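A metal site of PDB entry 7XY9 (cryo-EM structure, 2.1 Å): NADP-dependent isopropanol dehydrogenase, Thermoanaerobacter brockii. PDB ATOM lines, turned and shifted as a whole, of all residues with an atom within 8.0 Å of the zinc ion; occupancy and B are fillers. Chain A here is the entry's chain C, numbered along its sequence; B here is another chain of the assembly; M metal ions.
The backbone carbonyl oxygen (O) of Asp 156 sits at hydrogen-bond distance from the side-chain hydroxyl (OG1) of Thr 160 (2.8 Å).
SG of Cys 43 sits close to N of Ser 45, 3.6 Å away.
OD2 of Asp 46 is in hydrogen-bond range of N of Cys 43 (3.4 Å).
The side-chain carboxylate (OE2) of Glu 66 lies within salt-bridge range of the side-chain amino group (NZ) of Lys 352 (3.5 Å).
N of Ala 41 is in hydrogen-bond range of O of Glu 66 (3.2 Å).
The side-chain sulfur (SD) of Met 157 is in hydrogen-bond range of the side-chain amino group (NZ) of Lys 352 (3.4 Å).
Merely in contact with the zinc ion: Glu 66 (3.0 Å) and Met 157 (3.7 Å).
Of the 20 residues printed, 5 come within 4 Å of the zinc ion.
The zinc ion is bound by the side-chain carboxylate of Asp 156 (2.0 Å), a ring nitrogen (NE2) of His 65 (2.0 Å) and the side-chain sulfur of Cys 43 (2.4 Å).
The zinc ion has three donor atoms within binding distance.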
ATOM      1  N   ALA A  41      15.526  11.591  23.015  1.00  0.00           N
ATOM      2  CA  ALA A  41      15.984  11.333  24.378  1.00  0.00           C
ATOM      3  C   ALA A  41      16.554   9.925  24.473  1.00  0.00           C
ATOM      4  O   ALA A  41      15.846   8.944  24.143  1.00  0.00           O
ATOM      5  CB  ALA A  41      14.846  11.518  25.385  1.00  0.00           C
ATOM      6  N   PRO A  42      17.801   9.774  24.906  1.00  0.00           N
ATOM      7  CA  PRO A  42      18.338   8.431  25.156  1.00  0.00           C
ATOM      8  C   PRO A  42      17.673   7.778  26.351  1.00  0.00           C
ATOM      9  O   PRO A  42      17.144   8.437  27.245  1.00  0.00           O
ATOM     10  CB  PRO A  42      19.826   8.687  25.414  1.00  0.00           C
ATOM     11  CG  PRO A  42      19.887  10.097  25.900  1.00  0.00           C
ATOM     12  CD  PRO A  42      18.801  10.820  25.157  1.00  0.00           C
ATOM     13  N   CYS A  43      17.701   6.448  26.356  1.00  0.00           N
ATOM     14  CA  CYS A  43      17.077   5.657  27.412  1.00  0.00           C
ATOM     15  C   CYS A  43      18.084   4.674  27.987  1.00  0.00           C
ATOM     16  O   CYS A  43      19.109   4.376  27.374  1.00  0.00           O
ATOM     17  CB  CYS A  43      15.848   4.890  26.897  1.00  0.00           C
ATOM     18  SG  CYS A  43      14.824   4.154  28.180  1.00  0.00           S
ATOM     19  N   THR A  44      17.780   4.182  29.188  1.00  0.00           N
ATOM     20  CA  THR A  44      18.602   3.136  29.792  1.00  0.00           C
ATOM     21  C   THR A  44      18.535   1.848  28.990  1.00  0.00           C
ATOM     22  O   THR A  44      19.460   1.030  29.060  1.00  0.00           O
ATOM     23  CB  THR A  44      18.166   2.885  31.229  1.00  0.00           C
ATOM     24  OG1 THR A  44      16.739   2.717  31.285  1.00  0.00           O
ATOM     25  CG2 THR A  44      18.554   4.063  32.122  1.00  0.00           C
ATOM     26  N   SER A  45      17.455   1.642  28.233  1.00  0.00           N
ATOM     27  CA  SER A  45      17.326   0.451  27.411  1.00  0.00           C
ATOM     28  C   SER A  45      18.401   0.399  26.324  1.00  0.00           C
ATOM     29  O   SER A  45      18.945  -0.661  26.026  1.00  0.00           O
ATOM     30  CB  SER A  45      15.930   0.376  26.790  1.00  0.00           C
ATOM     31  OG  SER A  45      15.827   1.227  25.667  1.00  0.00           O
ATOM     32  N   ASP A  46      18.708   1.546  25.721  1.00  0.00           N
ATOM     33  CA  ASP A  46      19.777   1.599  24.717  1.00  0.00           C
ATOM     34  C   ASP A  46      21.107   1.194  25.330  1.00  0.00           C
ATOM     35  O   ASP A  46      21.887   0.454  24.718  1.00  0.00           O
ATOM     36  CB  ASP A  46      19.861   2.993  24.112  1.00  0.00           C
ATOM     37  CG  ASP A  46      18.608   3.387  23.365  1.00  0.00           C
ATOM     38  OD1 ASP A  46      18.087   2.569  22.584  1.00  0.00           O
ATOM     39  OD2 ASP A  46      18.145   4.530  23.550  1.00  0.00           O
ATOM     40  N   GLY A  64      17.893   4.466  19.781  1.00  0.00           N
ATOM     41  CA  GLY A  64      16.898   5.468  20.130  1.00  0.00           C
ATOM     42  C   GLY A  64      15.471   5.067  19.813  1.00  0.00           C
ATOM     43  O   GLY A  64      15.188   4.556  18.729  1.00  0.00           O
ATOM     44  N   HIS A  65      14.547   5.288  20.765  1.00  0.00           N
ATOM     45  CA  HIS A  65      13.139   5.009  20.509  1.00  0.00           C
ATOM     46  C   HIS A  65      12.205   6.040  21.144  1.00  0.00           C
ATOM     47  O   HIS A  65      11.024   5.749  21.338  1.00  0.00           O
ATOM     48  CB  HIS A  65      12.772   3.604  21.002  1.00  0.00           C
ATOM     49  CG  HIS A  65      12.771   3.460  22.495  1.00  0.00           C
ATOM     50  ND1 HIS A  65      12.015   2.499  23.143  1.00  0.00           N
ATOM     51  CD2 HIS A  65      13.425   4.135  23.460  1.00  0.00           C
ATOM     52  CE1 HIS A  65      12.207   2.608  24.450  1.00  0.00           C
ATOM     53  NE2 HIS A  65      13.059   3.589  24.668  1.00  0.00           N
ATOM     54  N   GLU A  66      12.693   7.239  21.449  1.00  0.00           N
ATOM     55  CA  GLU A  66      11.880   8.299  22.030  1.00  0.00           C
ATOM     56  C   GLU A  66      12.119   9.575  21.230  1.00  0.00           C
ATOM     57  O   GLU A  66      13.123  10.274  21.445  1.00  0.00           O
ATOM     58  CB  GLU A  66      12.196   8.527  23.506  1.00  0.00           C
ATOM     59  CG  GLU A  66      12.001   7.314  24.380  1.00  0.00           C
ATOM     60  CD  GLU A  66      12.793   7.403  25.664  1.00  0.00           C
ATOM     61  OE1 GLU A  66      13.988   7.059  25.650  1.00  0.00           O
ATOM     62  OE2 GLU A  66      12.213   7.818  26.695  1.00  0.00           O
ATOM     63  N   ALA A  91       6.988   4.822  21.326  1.00  0.00           N
ATOM     64  CA  ALA A  91       8.080   3.863  21.329  1.00  0.00           C
ATOM     65  C   ALA A  91       7.623   2.498  20.827  1.00  0.00           C
ATOM     66  O   ALA A  91       8.363   1.794  20.133  1.00  0.00           O
ATOM     67  CB  ALA A  91       8.685   3.745  22.732  1.00  0.00           C
ATOM     68  N   TRP A 116       7.476  -3.501  19.581  1.00  0.00           N
ATOM     69  CA  TRP A 116       8.789  -3.013  20.009  1.00  0.00           C
ATOM     70  C   TRP A 116       9.758  -3.227  18.860  1.00  0.00           C
ATOM     71  O   TRP A 116      10.449  -4.244  18.772  1.00  0.00           O
ATOM     72  CB  TRP A 116       9.236  -3.731  21.278  1.00  0.00           C
ATOM     73  CG  TRP A 116       8.490  -3.294  22.500  1.00  0.00           C
ATOM     74  CD1 TRP A 116       7.630  -4.036  23.245  1.00  0.00           C
ATOM     75  CD2 TRP A 116       8.517  -1.986  23.102  1.00  0.00           C
ATOM     76  NE1 TRP A 116       7.126  -3.289  24.282  1.00  0.00           N
ATOM     77  CE2 TRP A 116       7.661  -2.032  24.217  1.00  0.00           C
ATOM     78  CE3 TRP A 116       9.190  -0.801  22.820  1.00  0.00           C
ATOM     79  CZ2 TRP A 116       7.455  -0.925  25.039  1.00  0.00           C
ATOM     80  CZ3 TRP A 116       8.991   0.294  23.633  1.00  0.00           C
ATOM     81  CH2 TRP A 116       8.127   0.222  24.732  1.00  0.00           C
ATOM     82  N   SER A 119      15.101   0.351  17.378  1.00  0.00           N
ATOM     83  CA  SER A 119      16.380  -0.051  17.974  1.00  0.00           C
ATOM     84  C   SER A 119      16.367  -1.487  18.492  1.00  0.00           C
ATOM     85  O   SER A 119      17.211  -1.862  19.312  1.00  0.00           O
ATOM     86  CB  SER A 119      16.800   0.915  19.097  1.00  0.00           C
ATOM     87  OG  SER A 119      16.029   0.699  20.274  1.00  0.00           O
ATOM     88  N   PRO A 155       6.463   9.483  24.704  1.00  0.00           N
ATOM     89  CA  PRO A 155       6.497   8.189  23.986  1.00  0.00           C
ATOM     90  C   PRO A 155       6.828   6.974  24.848  1.00  0.00           C
ATOM     91  O   PRO A 155       6.264   5.899  24.617  1.00  0.00           O
ATOM     92  CB  PRO A 155       7.563   8.415  22.915  1.00  0.00           C
ATOM     93  CG  PRO A 155       7.547   9.882  22.686  1.00  0.00           C
ATOM     94  CD  PRO A 155       7.336  10.466  24.042  1.00  0.00           C
ATOM     95  N   ASP A 156       7.754   7.086  25.798  1.00  0.00           N
ATOM     96  CA  ASP A 156       8.140   5.929  26.600  1.00  0.00           C
ATOM     97  C   ASP A 156       7.894   6.108  28.091  1.00  0.00           C
ATOM     98  O   ASP A 156       7.167   5.301  28.691  1.00  0.00           O
ATOM     99  CB  ASP A 156       9.622   5.600  26.351  1.00  0.00           C
ATOM    100  CG  ASP A 156       9.983   4.192  26.759  1.00  0.00           C
ATOM    101  OD1 ASP A 156       9.079   3.339  26.834  1.00  0.00           O
ATOM    102  OD2 ASP A 156      11.181   3.928  27.007  1.00  0.00           O
ATOM    103  N   MET A 157       8.452   7.149  28.707  1.00  0.00           N
ATOM    104  CA  MET A 157       8.435   7.241  30.167  1.00  0.00           C
ATOM    105  C   MET A 157       7.015   7.447  30.686  1.00  0.00           C
ATOM    106  O   MET A 157       6.571   6.738  31.598  1.00  0.00           O
ATOM    107  CB  MET A 157       9.354   8.366  30.643  1.00  0.00           C
ATOM    108  CG  MET A 157      10.689   8.420  29.923  1.00  0.00           C
ATOM    109  SD  MET A 157      11.913   7.356  30.696  1.00  0.00           S
ATOM    110  CE  MET A 157      11.829   5.914  29.640  1.00  0.00           C
ATOM    111  N   THR A 160       4.759   4.315  30.066  1.00  0.00           N
ATOM    112  CA  THR A 160       5.099   3.179  30.908  1.00  0.00           C
ATOM    113  C   THR A 160       4.684   3.413  32.362  1.00  0.00           C
ATOM    114  O   THR A 160       4.062   2.548  32.979  1.00  0.00           O
ATOM    115  CB  THR A 160       6.597   2.881  30.826  1.00  0.00           C
ATOM    116  OG1 THR A 160       6.963   2.644  29.461  1.00  0.00           O
ATOM    117  CG2 THR A 160       6.957   1.661  31.654  1.00  0.00           C
ATOM    118  N   VAL A 184      10.750   6.523  35.005  1.00  0.00           N
ATOM    119  CA  VAL A 184       9.551   5.699  34.957  1.00  0.00           C
ATOM    120  C   VAL A 184       8.846   5.691  36.303  1.00  0.00           C
ATOM    121  O   VAL A 184       7.623   5.746  36.373  1.00  0.00           O
ATOM    122  CB  VAL A 184       9.909   4.268  34.486  1.00  0.00           C
ATOM    123  CG1 VAL A 184       8.733   3.321  34.686  1.00  0.00           C
ATOM    124  CG2 VAL A 184      10.321   4.282  33.015  1.00  0.00           C
ATOM    125  N   TYR A 273      11.567  -2.593  33.049  1.00  0.00           N
ATOM    126  CA  TYR A 273      12.096  -3.325  31.905  1.00  0.00           C
ATOM    127  C   TYR A 273      13.509  -3.816  32.176  1.00  0.00           C
ATOM    128  O   TYR A 273      14.349  -3.077  32.691  1.00  0.00           O
ATOM    129  CB  TYR A 273      12.083  -2.425  30.657  1.00  0.00           C
ATOM    130  CG  TYR A 273      13.014  -2.903  29.563  1.00  0.00           C
ATOM    131  CD1 TYR A 273      12.692  -4.016  28.793  1.00  0.00           C
ATOM    132  CD2 TYR A 273      14.204  -2.247  29.305  1.00  0.00           C
ATOM    133  CE1 TYR A 273      13.540  -4.448  27.794  1.00  0.00           C
ATOM    134  CE2 TYR A 273      15.058  -2.684  28.317  1.00  0.00           C
ATOM    135  CZ  TYR A 273      14.719  -3.781  27.554  1.00  0.00           C
ATOM    136  OH  TYR A 273      15.564  -4.214  26.564  1.00  0.00           O
ATOM    137  N   LYS A 352      16.965  12.791  33.042  1.00  0.00           N
ATOM    138  CA  LYS A 352      16.727  12.481  31.636  1.00  0.00           C
ATOM    139  C   LYS A 352      17.281  13.596  30.739  1.00  0.00           C
ATOM    140  O   LYS A 352      16.854  14.752  30.853  1.00  0.00           O
ATOM    141  CB  LYS A 352      15.232  12.282  31.381  1.00  0.00           C
ATOM    142  CG  LYS A 352      14.926  11.539  30.097  1.00  0.00           C
ATOM    143  CD  LYS A 352      14.816  10.039  30.313  1.00  0.00           C
ATOM    144  CE  LYS A 352      14.417   9.335  29.025  1.00  0.00           C
ATOM    145  NZ  LYS A 352      14.809   7.903  29.018  1.00  0.00           N
ATOM    146  N   TRP B 287      11.657  -7.220  25.570  1.00  0.00           N
ATOM    147  CA  TRP B 287      10.929  -6.874  24.351  1.00  0.00           C
ATOM    148  C   TRP B 287      10.605  -8.117  23.525  1.00  0.00           C
ATOM    149  O   TRP B 287       9.511  -8.204  22.946  1.00  0.00           O
ATOM    150  CB  TRP B 287      11.737  -5.880  23.522  1.00  0.00           C
ATOM    151  CG  TRP B 287      11.802  -4.506  24.101  1.00  0.00           C
ATOM    152  CD1 TRP B 287      10.923  -3.943  24.978  1.00  0.00           C
ATOM    153  CD2 TRP B 287      12.793  -3.509  23.827  1.00  0.00           C
ATOM    154  NE1 TRP B 287      11.309  -2.654  25.270  1.00  0.00           N
ATOM    155  CE2 TRP B 287      12.456  -2.362  24.569  1.00  0.00           C
ATOM    156  CE3 TRP B 287      13.929  -3.472  23.011  1.00  0.00           C
ATOM    157  CZ2 TRP B 287      13.220  -1.198  24.546  1.00  0.00           C
ATOM    158  CZ3 TRP B 287      14.690  -2.318  22.986  1.00  0.00           C
ATOM    159  CH2 TRP B 287      14.326  -1.196  23.739  1.00  0.00           C
HETATM  160 ZN    ZN M   1      13.083   4.310  26.577  1.00  0.00          ZN
